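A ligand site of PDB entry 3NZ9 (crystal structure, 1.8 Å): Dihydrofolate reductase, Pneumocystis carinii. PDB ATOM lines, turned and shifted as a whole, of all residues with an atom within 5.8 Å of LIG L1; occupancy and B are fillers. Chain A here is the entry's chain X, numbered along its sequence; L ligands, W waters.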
ATOM      1  N   ILE A  10      23.257  -6.615  11.084  1.00  0.00           N
ATOM      2  CA  ILE A  10      24.552  -7.275  11.309  1.00  0.00           C
ATOM      3  C   ILE A  10      24.703  -8.402  10.229  1.00  0.00           C
ATOM      4  O   ILE A  10      23.757  -9.182   9.959  1.00  0.00           O
ATOM      5  CB  ILE A  10      24.748  -7.848  12.764  1.00  0.00           C
ATOM      6  CG1 ILE A  10      26.173  -8.460  12.909  1.00  0.00           C
ATOM      7  CG2 ILE A  10      23.614  -8.822  13.153  1.00  0.00           C
ATOM      8  CD1 ILE A  10      26.679  -8.634  14.428  1.00  0.00           C
ATOM      9  N   VAL A  11      25.869  -8.426   9.626  1.00  0.00           N
ATOM     10  CA  VAL A  11      26.126  -9.204   8.390  1.00  0.00           C
ATOM     11  C   VAL A  11      27.632  -9.484   8.266  1.00  0.00           C
ATOM     12  O   VAL A  11      28.505  -8.704   8.677  1.00  0.00           O
ATOM     13  CB  VAL A  11      25.601  -8.436   7.077  1.00  0.00           C
ATOM     14  CG1 VAL A  11      26.380  -7.151   6.800  1.00  0.00           C
ATOM     15  CG2 VAL A  11      25.643  -9.360   5.843  1.00  0.00           C
ATOM     16  N   ALA A  12      27.939 -10.653   7.674  1.00  0.00           N
ATOM     17  CA  ALA A  12      29.302 -11.049   7.247  1.00  0.00           C
ATOM     18  C   ALA A  12      29.190 -11.149   5.741  1.00  0.00           C
ATOM     19  O   ALA A  12      28.215 -11.797   5.203  1.00  0.00           O
ATOM     20  CB  ALA A  12      29.662 -12.382   7.826  1.00  0.00           C
ATOM     21  N   SER A  24      23.110 -21.664   3.288  1.00  0.00           N
ATOM     22  CA  SER A  24      24.003 -21.627   4.465  1.00  0.00           C
ATOM     23  C   SER A  24      25.122 -20.581   4.236  1.00  0.00           C
ATOM     24  O   SER A  24      25.101 -19.876   3.245  1.00  0.00           O
ATOM     25  CB  SER A  24      24.617 -23.006   4.748  1.00  0.00           C
ATOM     26  OG  SER A  24      25.714 -23.235   3.889  1.00  0.00           O
ATOM     27  N   LEU A  25      26.076 -20.487   5.145  1.00  0.00           N
ATOM     28  CA  LEU A  25      27.260 -19.636   4.943  1.00  0.00           C
ATOM     29  C   LEU A  25      28.361 -20.373   4.223  1.00  0.00           C
ATOM     30  O   LEU A  25      28.760 -21.455   4.677  1.00  0.00           O
ATOM     31  CB  LEU A  25      27.809 -19.140   6.299  1.00  0.00           C
ATOM     32  CG  LEU A  25      26.672 -18.446   7.054  1.00  0.00           C
ATOM     33  CD1 LEU A  25      27.094 -18.137   8.471  1.00  0.00           C
ATOM     34  CD2 LEU A  25      26.323 -17.166   6.301  1.00  0.00           C
ATOM     35  N   GLU A  32      34.211 -15.514  14.156  1.00  0.00           N
ATOM     36  CA  GLU A  32      33.270 -14.588  13.506  1.00  0.00           C
ATOM     37  C   GLU A  32      31.878 -14.830  14.101  1.00  0.00           C
ATOM     38  O   GLU A  32      31.174 -13.877  14.516  1.00  0.00           O
ATOM     39  CB  GLU A  32      33.272 -14.755  11.985  1.00  0.00           C
ATOM     40  CG  GLU A  32      32.867 -13.455  11.232  1.00  0.00           C
ATOM     41  CD  GLU A  32      31.388 -13.062  11.488  1.00  0.00           C
ATOM     42  OE1 GLU A  32      30.537 -13.968  11.478  1.00  0.00           O
ATOM     43  OE2 GLU A  32      31.065 -11.872  11.745  1.00  0.00           O
ATOM     44  N   ILE A  33      31.493 -16.098  14.167  1.00  0.00           N
ATOM     45  CA  ILE A  33      30.198 -16.419  14.851  1.00  0.00           C
ATOM     46  C   ILE A  33      30.175 -15.943  16.325  1.00  0.00           C
ATOM     47  O   ILE A  33      29.159 -15.419  16.814  1.00  0.00           O
ATOM     48  CB  ILE A  33      29.820 -17.899  14.720  1.00  0.00           C
ATOM     49  CG1 ILE A  33      29.414 -18.211  13.288  1.00  0.00           C
ATOM     50  CG2 ILE A  33      28.655 -18.223  15.713  1.00  0.00           C
ATOM     51  CD1 ILE A  33      29.045 -19.657  13.072  1.00  0.00           C
ATOM     52  N   TYR A  35      31.786 -13.414  17.598  1.00  0.00           N
ATOM     53  CA  TYR A  35      31.532 -11.963  17.504  1.00  0.00           C
ATOM     54  C   TYR A  35      30.015 -11.647  17.310  1.00  0.00           C
ATOM     55  O   TYR A  35      29.463 -10.781  18.000  1.00  0.00           O
ATOM     56  CB  TYR A  35      32.350 -11.381  16.342  1.00  0.00           C
ATOM     57  CG  TYR A  35      32.139  -9.903  16.075  1.00  0.00           C
ATOM     58  CD1 TYR A  35      32.827  -8.927  16.804  1.00  0.00           C
ATOM     59  CD2 TYR A  35      31.265  -9.484  15.086  1.00  0.00           C
ATOM     60  CE1 TYR A  35      32.650  -7.555  16.567  1.00  0.00           C
ATOM     61  CE2 TYR A  35      31.115  -8.096  14.822  1.00  0.00           C
ATOM     62  CZ  TYR A  35      31.793  -7.156  15.554  1.00  0.00           C
ATOM     63  OH  TYR A  35      31.584  -5.823  15.281  1.00  0.00           O
ATOM     64  N   PHE A  36      29.408 -12.284  16.316  1.00  0.00           N
ATOM     65  CA  PHE A  36      27.966 -12.112  16.098  1.00  0.00           C
ATOM     66  C   PHE A  36      27.217 -12.355  17.418  1.00  0.00           C
ATOM     67  O   PHE A  36      26.376 -11.550  17.800  1.00  0.00           O
ATOM     68  CB  PHE A  36      27.530 -13.091  15.014  1.00  0.00           C
ATOM     69  CG  PHE A  36      26.080 -13.274  14.927  1.00  0.00           C
ATOM     70  CD1 PHE A  36      25.291 -12.346  14.225  1.00  0.00           C
ATOM     71  CD2 PHE A  36      25.467 -14.330  15.573  1.00  0.00           C
ATOM     72  CE1 PHE A  36      23.881 -12.556  14.148  1.00  0.00           C
ATOM     73  CE2 PHE A  36      24.079 -14.529  15.498  1.00  0.00           C
ATOM     74  CZ  PHE A  36      23.294 -13.656  14.750  1.00  0.00           C
ATOM     75  N   LYS A  37      27.556 -13.444  18.111  1.00  0.00           N
ATOM     76  CA  LYS A  37      26.815 -13.804  19.351  1.00  0.00           C
ATOM     77  C   LYS A  37      27.106 -12.714  20.388  1.00  0.00           C
ATOM     78  O   LYS A  37      26.196 -12.196  21.065  1.00  0.00           O
ATOM     79  CB  LYS A  37      27.238 -15.215  19.826  1.00  0.00           C
ATOM     80  CG  LYS A  37      26.523 -15.769  21.071  1.00  0.00           C
ATOM     81  CD  LYS A  37      27.127 -17.157  21.413  1.00  0.00           C
ATOM     82  CE  LYS A  37      26.662 -17.628  22.816  1.00  0.00           C
ATOM     83  NZ  LYS A  37      27.649 -18.576  23.487  1.00  0.00           N
ATOM     84  N   THR A  61      16.713 -17.728   6.631  1.00  0.00           N
ATOM     85  CA  THR A  61      17.778 -17.704   7.678  1.00  0.00           C
ATOM     86  C   THR A  61      17.472 -18.536   8.921  1.00  0.00           C
ATOM     87  O   THR A  61      18.365 -19.194   9.553  1.00  0.00           O
ATOM     88  CB  THR A  61      18.073 -16.173   8.066  1.00  0.00           C
ATOM     89  OG1 THR A  61      18.510 -15.518   6.888  1.00  0.00           O
ATOM     90  CG2 THR A  61      19.086 -16.046   9.151  1.00  0.00           C
ATOM     91  N   SER A  64      18.129 -21.948   7.918  1.00  0.00           N
ATOM     92  CA  SER A  64      19.584 -22.020   7.677  1.00  0.00           C
ATOM     93  C   SER A  64      20.381 -22.333   8.906  1.00  0.00           C
ATOM     94  O   SER A  64      21.413 -22.961   8.821  1.00  0.00           O
ATOM     95  CB  SER A  64      20.121 -20.683   7.138  1.00  0.00           C
ATOM     96  OG  SER A  64      21.540 -20.739   6.950  1.00  0.00           O
ATOM     97  N   ILE A  65      19.933 -21.839  10.041  1.00  0.00           N
ATOM     98  CA  ILE A  65      20.635 -22.054  11.313  1.00  0.00           C
ATOM     99  C   ILE A  65      20.427 -23.516  11.772  1.00  0.00           C
ATOM    100  O   ILE A  65      19.276 -24.005  11.746  1.00  0.00           O
ATOM    101  CB  ILE A  65      20.141 -21.083  12.382  1.00  0.00           C
ATOM    102  CG1 ILE A  65      20.398 -19.611  11.930  1.00  0.00           C
ATOM    103  CG2 ILE A  65      20.803 -21.348  13.702  1.00  0.00           C
ATOM    104  CD1 ILE A  65      19.966 -18.563  12.947  1.00  0.00           C
ATOM    105  N   PRO A  66      21.524 -24.221  12.148  1.00  0.00           N
ATOM    106  CA  PRO A  66      21.394 -25.615  12.593  1.00  0.00           C
ATOM    107  C   PRO A  66      20.334 -25.684  13.672  1.00  0.00           C
ATOM    108  O   PRO A  66      20.326 -24.833  14.578  1.00  0.00           O
ATOM    109  CB  PRO A  66      22.797 -25.941  13.176  1.00  0.00           C
ATOM    110  CG  PRO A  66      23.721 -25.100  12.364  1.00  0.00           C
ATOM    111  CD  PRO A  66      22.935 -23.777  12.108  1.00  0.00           C
ATOM    112  N   PHE A  69      20.829 -24.754  17.249  1.00  0.00           N
ATOM    113  CA  PHE A  69      21.154 -23.410  17.712  1.00  0.00           C
ATOM    114  C   PHE A  69      19.910 -22.465  17.825  1.00  0.00           C
ATOM    115  O   PHE A  69      20.033 -21.286  18.159  1.00  0.00           O
ATOM    116  CB  PHE A  69      22.287 -22.843  16.855  1.00  0.00           C
ATOM    117  CG  PHE A  69      23.621 -23.554  17.051  1.00  0.00           C
ATOM    118  CD1 PHE A  69      24.240 -23.572  18.310  1.00  0.00           C
ATOM    119  CD2 PHE A  69      24.242 -24.220  15.993  1.00  0.00           C
ATOM    120  CE1 PHE A  69      25.461 -24.251  18.502  1.00  0.00           C
ATOM    121  CE2 PHE A  69      25.459 -24.889  16.166  1.00  0.00           C
ATOM    122  CZ  PHE A  69      26.070 -24.910  17.430  1.00  0.00           C
ATOM    123  N   LEU A  72      17.885 -18.526  18.844  1.00  0.00           N
ATOM    124  CA  LEU A  72      19.151 -18.003  19.279  1.00  0.00           C
ATOM    125  C   LEU A  72      19.080 -17.590  20.718  1.00  0.00           C
ATOM    126  O   LEU A  72      18.312 -16.706  21.107  1.00  0.00           O
ATOM    127  CB  LEU A  72      19.645 -16.848  18.378  1.00  0.00           C
ATOM    128  CG  LEU A  72      19.968 -17.208  16.902  1.00  0.00           C
ATOM    129  CD1 LEU A  72      20.214 -15.906  16.068  1.00  0.00           C
ATOM    130  CD2 LEU A  72      21.173 -18.163  16.760  1.00  0.00           C
ATOM    131  N   ARG A  75      18.348 -14.139  23.347  1.00  0.00           N
ATOM    132  CA  ARG A  75      17.842 -12.983  22.602  1.00  0.00           C
ATOM    133  C   ARG A  75      16.380 -13.264  22.296  1.00  0.00           C
ATOM    134  O   ARG A  75      15.986 -14.440  22.084  1.00  0.00           O
ATOM    135  CB  ARG A  75      18.653 -12.814  21.319  1.00  0.00           C
ATOM    136  CG  ARG A  75      20.041 -12.256  21.592  1.00  0.00           C
ATOM    137  CD  ARG A  75      21.022 -12.853  20.541  1.00  0.00           C
ATOM    138  NE  ARG A  75      21.331 -14.285  20.877  1.00  0.00           N
ATOM    139  CZ  ARG A  75      22.274 -15.000  20.294  1.00  0.00           C
ATOM    140  NH1 ARG A  75      22.994 -14.478  19.277  1.00  0.00           N
ATOM    141  NH2 ARG A  75      22.504 -16.250  20.731  1.00  0.00           N
ATOM    142  N   VAL A 122      18.658  -6.775  12.821  1.00  0.00           N
ATOM    143  CA  VAL A 122      18.242  -7.566  11.664  1.00  0.00           C
ATOM    144  C   VAL A 122      19.425  -8.409  11.293  1.00  0.00           C
ATOM    145  O   VAL A 122      20.540  -7.918  11.101  1.00  0.00           O
ATOM    146  CB  VAL A 122      17.863  -6.638  10.508  1.00  0.00           C
ATOM    147  CG1 VAL A 122      17.656  -7.417   9.176  1.00  0.00           C
ATOM    148  CG2 VAL A 122      16.568  -5.787  10.960  1.00  0.00           C
ATOM    149  N   ILE A 123      19.234  -9.715  11.253  1.00  0.00           N
ATOM    150  CA  ILE A 123      20.392 -10.562  11.120  1.00  0.00           C
ATOM    151  C   ILE A 123      20.378 -11.356   9.832  1.00  0.00           C
ATOM    152  O   ILE A 123      21.255 -12.215   9.656  1.00  0.00           O
ATOM    153  CB  ILE A 123      20.471 -11.606  12.279  1.00  0.00           C
ATOM    154  CG1 ILE A 123      19.255 -12.542  12.297  1.00  0.00           C
ATOM    155  CG2 ILE A 123      20.518 -10.909  13.602  1.00  0.00           C
ATOM    156  CD1 ILE A 123      19.555 -13.918  13.013  1.00  0.00           C
ATOM    157  N   GLY A 124      19.430 -11.048   8.957  1.00  0.00           N
ATOM    158  CA  GLY A 124      19.407 -11.644   7.596  1.00  0.00           C
ATOM    159  C   GLY A 124      18.085 -12.297   7.251  1.00  0.00           C
ATOM    160  O   GLY A 124      17.194 -12.312   8.097  1.00  0.00           O
ATOM    161  N   TYR A 129      17.251  -8.034   4.732  1.00  0.00           N
ATOM    162  CA  TYR A 129      18.214  -6.942   4.678  1.00  0.00           C
ATOM    163  C   TYR A 129      17.732  -5.874   3.718  1.00  0.00           C
ATOM    164  O   TYR A 129      17.879  -4.696   3.991  1.00  0.00           O
ATOM    165  CB  TYR A 129      19.566  -7.417   4.165  1.00  0.00           C
ATOM    166  CG  TYR A 129      20.399  -8.240   5.162  1.00  0.00           C
ATOM    167  CD1 TYR A 129      20.466  -7.893   6.525  1.00  0.00           C
ATOM    168  CD2 TYR A 129      21.214  -9.266   4.703  1.00  0.00           C
ATOM    169  CE1 TYR A 129      21.278  -8.603   7.416  1.00  0.00           C
ATOM    170  CE2 TYR A 129      22.058  -9.955   5.579  1.00  0.00           C
ATOM    171  CZ  TYR A 129      22.071  -9.633   6.919  1.00  0.00           C
ATOM    172  OH  TYR A 129      22.929 -10.341   7.746  1.00  0.00           O
ATOM    173  N   MET A 142      26.671  -3.482  11.188  1.00  0.00           N
ATOM    174  CA  MET A 142      27.875  -4.117  11.801  1.00  0.00           C
ATOM    175  C   MET A 142      28.287  -5.120  10.700  1.00  0.00           C
ATOM    176  O   MET A 142      27.583  -6.083  10.472  1.00  0.00           O
ATOM    177  CB  MET A 142      27.500  -4.851  13.110  1.00  0.00           C
ATOM    178  CG  MET A 142      26.796  -3.962  14.168  1.00  0.00           C
ATOM    179  SD  MET A 142      27.768  -2.477  14.568  1.00  0.00           S
ATOM    180  CE  MET A 142      29.119  -3.204  15.404  1.00  0.00           C
ATOM    181  N   ALA A 143      29.356  -4.796   9.950  1.00  0.00           N
ATOM    182  CA  ALA A 143      29.684  -5.635   8.751  1.00  0.00           C
ATOM    183  C   ALA A 143      30.949  -6.341   9.059  1.00  0.00           C
ATOM    184  O   ALA A 143      31.917  -5.692   9.466  1.00  0.00           O
ATOM    185  CB  ALA A 143      29.862  -4.753   7.552  1.00  0.00           C
ATOM    186  N   THR A 144      30.991  -7.643   8.819  1.00  0.00           N
ATOM    187  CA  THR A 144      32.303  -8.311   8.765  1.00  0.00           C
ATOM    188  C   THR A 144      32.689  -8.475   7.309  1.00  0.00           C
ATOM    189  O   THR A 144      31.976  -9.138   6.566  1.00  0.00           O
ATOM    190  CB  THR A 144      32.213  -9.659   9.463  1.00  0.00           C
ATOM    191  OG1 THR A 144      31.775  -9.429  10.815  1.00  0.00           O
ATOM    192  CG2 THR A 144      33.600 -10.384   9.457  1.00  0.00           C
HETATM  193  N1  LIG L   1      26.196 -11.652  10.926  1.00  0.00           N
HETATM  194  C1  LIG L   1      27.475 -11.998  11.116  1.00  0.00           C
HETATM  195  N2  LIG L   1      27.784 -13.289  11.275  1.00  0.00           N
HETATM  196  C2  LIG L   1      26.812 -14.224  11.291  1.00  0.00           C
HETATM  197  C3  LIG L   1      25.444 -13.870  11.163  1.00  0.00           C
HETATM  198  C4  LIG L   1      25.150 -12.488  10.941  1.00  0.00           C
HETATM  199  C5  LIG L   1      27.394 -21.805  19.846  1.00  0.00           C
HETATM  200  C6  LIG L   1      22.340 -17.718   9.124  1.00  0.00           C
HETATM  201  C7  LIG L   1      22.984 -14.742  11.138  1.00  0.00           C
HETATM  202  N3  LIG L   1      28.477 -11.057  11.093  1.00  0.00           N
HETATM  203  N4  LIG L   1      23.931 -11.971  10.734  1.00  0.00           N
HETATM  204  O1  LIG L   1      24.556 -19.764  17.727  1.00  0.00           O
HETATM  205  C8  LIG L   1      25.208 -21.196  10.600  1.00  0.00           C
HETATM  206  C9  LIG L   1      24.611 -20.436   9.589  1.00  0.00           C
HETATM  207  C10 LIG L   1      26.299 -16.479  11.552  1.00  0.00           C
HETATM  208  C11 LIG L   1      24.924 -19.380  12.163  1.00  0.00           C
HETATM  209  C12 LIG L   1      27.578 -21.167  18.449  1.00  0.00           C
HETATM  210  C13 LIG L   1      25.725 -21.282  15.300  1.00  0.00           C
HETATM  211  C14 LIG L   1      25.036 -21.178  13.961  1.00  0.00           C
HETATM  212  C15 LIG L   1      26.007 -19.899  15.858  1.00  0.00           C
HETATM  213  C16 LIG L   1      23.874 -17.282  11.547  1.00  0.00           C
HETATM  214  N5  LIG L   1      27.212 -15.498  11.468  1.00  0.00           N
HETATM  215  O2  LIG L   1      23.551 -18.392   8.843  1.00  0.00           O
HETATM  216  O3  LIG L   1      26.755 -19.952  18.306  1.00  0.00           O
HETATM  217  O4  LIG L   1      25.945 -21.424  12.844  1.00  0.00           O
HETATM  218  C17 LIG L   1      25.726 -19.897  17.368  1.00  0.00           C
HETATM  219  C18 LIG L   1      25.363 -20.681  11.868  1.00  0.00           C
HETATM  220  C19 LIG L   1      24.498 -14.896  11.264  1.00  0.00           C
HETATM  221  C20 LIG L   1      24.945 -16.193  11.446  1.00  0.00           C
HETATM  222  C21 LIG L   1      24.342 -18.638  11.145  1.00  0.00           C
HETATM  223  C22 LIG L   1      24.139 -19.147   9.863  1.00  0.00           C
HETATM  224  P1  LG2 L   2      15.788 -14.573   4.092  1.00  0.00           P
HETATM  225  O1  LG2 L   2      16.242 -15.193   5.357  1.00  0.00           O
HETATM  226  O2  LG2 L   2      15.611 -13.064   3.979  1.00  0.00           O
HETATM  227  O3  LG2 L   2      14.223 -15.155   4.018  1.00  0.00           O
HETATM  228  C1  LG2 L   2      13.557 -14.826   2.832  1.00  0.00           C
HETATM  229  C2  LG2 L   2      12.197 -15.152   3.206  1.00  0.00           C
HETATM  230  O4  LG2 L   2      11.957 -14.586   4.624  1.00  0.00           O
HETATM  231  C3  LG2 L   2      10.997 -14.728   2.372  1.00  0.00           C
HETATM  232  O5  LG2 L   2      10.815 -15.637   1.283  1.00  0.00           O
HETATM  233  C4  LG2 L   2      10.246 -15.183   3.599  1.00  0.00           C
HETATM  234  O6  LG2 L   2       8.945 -15.208   3.610  1.00  0.00           O
HETATM  235  C5  LG2 L   2      10.673 -14.040   4.568  1.00  0.00           C
HETATM  236  N1  LG2 L   2      10.829 -12.447   4.326  1.00  0.00           N
HETATM  237  C6  LG2 L   2      11.996 -11.762   4.137  1.00  0.00           C
HETATM  238  N2  LG2 L   2      11.806 -10.438   4.009  1.00  0.00           N
HETATM  239  C7  LG2 L   2      10.482 -10.234   4.183  1.00  0.00           C
HETATM  240  C8  LG2 L   2       9.653  -9.097   4.185  1.00  0.00           C
HETATM  241  N3  LG2 L   2      10.118  -7.841   3.980  1.00  0.00           N
HETATM  242  N4  LG2 L   2       8.320  -9.267   4.397  1.00  0.00           N
HETATM  243  C9  LG2 L   2       7.786 -10.477   4.597  1.00  0.00           C
HETATM  244  N5  LG2 L   2       8.531 -11.584   4.596  1.00  0.00           N
HETATM  245  C10 LG2 L   2       9.873 -11.497   4.390  1.00  0.00           C
HETATM  246  O7  LG2 L   2      16.371 -15.338   2.794  1.00  0.00           O
HETATM  247  P2  LG2 L   2      17.414 -14.912   1.621  1.00  0.00           P
HETATM  248  O8  LG2 L   2      17.186 -13.582   1.016  1.00  0.00           O
HETATM  249  O9  LG2 L   2      17.272 -16.139   0.725  1.00  0.00           O
HETATM  250  O10 LG2 L   2      18.848 -14.985   2.349  1.00  0.00           O
HETATM  251  C11 LG2 L   2      19.226 -16.210   2.983  1.00  0.00           C
HETATM  252  C12 LG2 L   2      20.670 -16.598   2.632  1.00  0.00           C
HETATM  253  O11 LG2 L   2      21.352 -15.591   3.451  1.00  0.00           O
HETATM  254  C13 LG2 L   2      21.139 -17.962   3.150  1.00  0.00           C
HETATM  255  O12 LG2 L   2      22.286 -18.409   2.360  1.00  0.00           O
HETATM  256  C14 LG2 L   2      21.671 -17.615   4.527  1.00  0.00           C
HETATM  257  O13 LG2 L   2      22.693 -18.558   4.896  1.00  0.00           O
HETATM  258  C15 LG2 L   2      22.338 -16.275   4.202  1.00  0.00           C
HETATM  259  N6  LG2 L   2      22.656 -15.411   5.364  1.00  0.00           N
HETATM  260  C16 LG2 L   2      23.932 -14.802   5.407  1.00  0.00           C
HETATM  261  C17 LG2 L   2      24.216 -14.002   6.495  1.00  0.00           C
HETATM  262  C18 LG2 L   2      25.608 -13.348   6.633  1.00  0.00           C
HETATM  263  O14 LG2 L   2      25.784 -12.582   7.585  1.00  0.00           O
HETATM  264  N7  LG2 L   2      26.551 -13.841   5.764  1.00  0.00           N
HETATM  265  C19 LG2 L   2      23.251 -13.763   7.516  1.00  0.00           C
HETATM  266  C20 LG2 L   2      21.994 -14.359   7.492  1.00  0.00           C
HETATM  267  C21 LG2 L   2      21.683 -15.166   6.394  1.00  0.00           C
HETATM  268  P3  LG2 L   2       7.929 -16.281   2.930  1.00  0.00           P
HETATM  269  O15 LG2 L   2       7.801 -17.263   4.190  1.00  0.00           O
HETATM  270  O16 LG2 L   2       8.716 -17.025   1.714  1.00  0.00           O
HETATM  271  O17 LG2 L   2       6.855 -15.278   2.550  1.00  0.00           O
HETATM  272  O   HOH W   1      29.879 -16.144   9.605  1.00  0.00           O
HETATM  273  O   HOH W   2      29.637  -7.831  11.673  1.00  0.00           O
HETATM  274  O   HOH W   3      24.625 -16.860  18.442  1.00  0.00           O
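A nitrogen (N3) of LIG L1 lies within hydrogen-bond range of the side-chain carboxylate (OE2) of Glu 32 (2.8 Å).
The backbone carbonyl oxygen of Ile 123 lies within hydrogen-bond range of a nitrogen (N4) of LIG L1 (2.9 Å).
The backbone carbonyl oxygen (O) of Ile 10 is in hydrogen-bond range of a nitrogen (N4) of LIG L1, at 2.9 Å.
N1 of LIG L1 is in hydrogen-bond range of N of Val 11 (3.5 Å).
O of Val 11 sits close to N3 of LIG L1 (3.4 Å).
The backbone NH of Ala 12 sits at hydrogen-bond distance from an oxygen (O14) of LG2 L2 (2.9 Å).
A nitrogen (N7) of LG2 L2 sits at hydrogen-bond distance from the backbone carbonyl oxygen (O) of Ala 12, 2.7 Å away.
The side-chain hydroxyl (OG) of Ser 64 is in hydrogen-bond range of an oxygen (O13) of LG2 L2 (3.2 Å).
The backbone NH (N) of Thr 61 lies within hydrogen-bond range of an oxygen (O1) of LG2 L2 (2.9 Å).
OG1 of Thr 61 is in hydrogen-bond range of O1 of LG2 L2, at 2.8 Å.
The backbone NH (N) of Ser 24 sits at hydrogen-bond distance from an oxygen (O12) of LG2 L2.
O of Ser 24 lies within hydrogen-bond range of O13 of LG2 L2.
OE2 of Glu 32 lies within hydrogen-bond range of OG1 of Thr 144 (2.7 Å).
The side-chain hydroxyl of Tyr 129 is in hydrogen-bond range of the backbone carbonyl oxygen of Ile 123 (3.2 Å).
The backbone carbonyl oxygen (O) of Ile 10 sits at hydrogen-bond distance from the side-chain hydroxyl (OH) of Tyr 129, 2.6 Å away.
N of Ile 10 is in hydrogen-bond range of O of Val 122 (3.0 Å).
The backbone NH (N) of Thr 144 lies within hydrogen-bond range of the backbone carbonyl oxygen (O) of Val 11 (2.7 Å).
N of Val 11 lies within hydrogen-bond range of O of Met 142 (3.0 Å).
The backbone NH (N) of Ala 12 lies close to a nitrogen (N3) of LIG L1 (3.5 Å).
Merely in contact with LIG L1: Ile 33, Phe 36, Phe 69, Leu 25, Tyr 129, Ser 64, Thr 61, Thr 144, Pro 66, Leu 72 and Ile 65.
Hydrophobic or aromatic side chains that line LIG L1: Ile 10, Ala 12, Leu 25, Ile 33, Phe 36, Ile 65, Pro 66, Phe 69, Leu 72 and Ile 123.
Water W3 bridges O1 of LIG L1 (3.0 Å) and NH1 of Arg 75 (3.0 Å).
Water W1 lies within hydrogen-bond range of OE1 of Glu 32 (2.9 Å) and N5 of LIG L1 (3.3 Å).
Water W2 lies within hydrogen-bond range of OG1 of Thr 144, O of Met 142, O of Val 11 and N3 of LIG L1.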
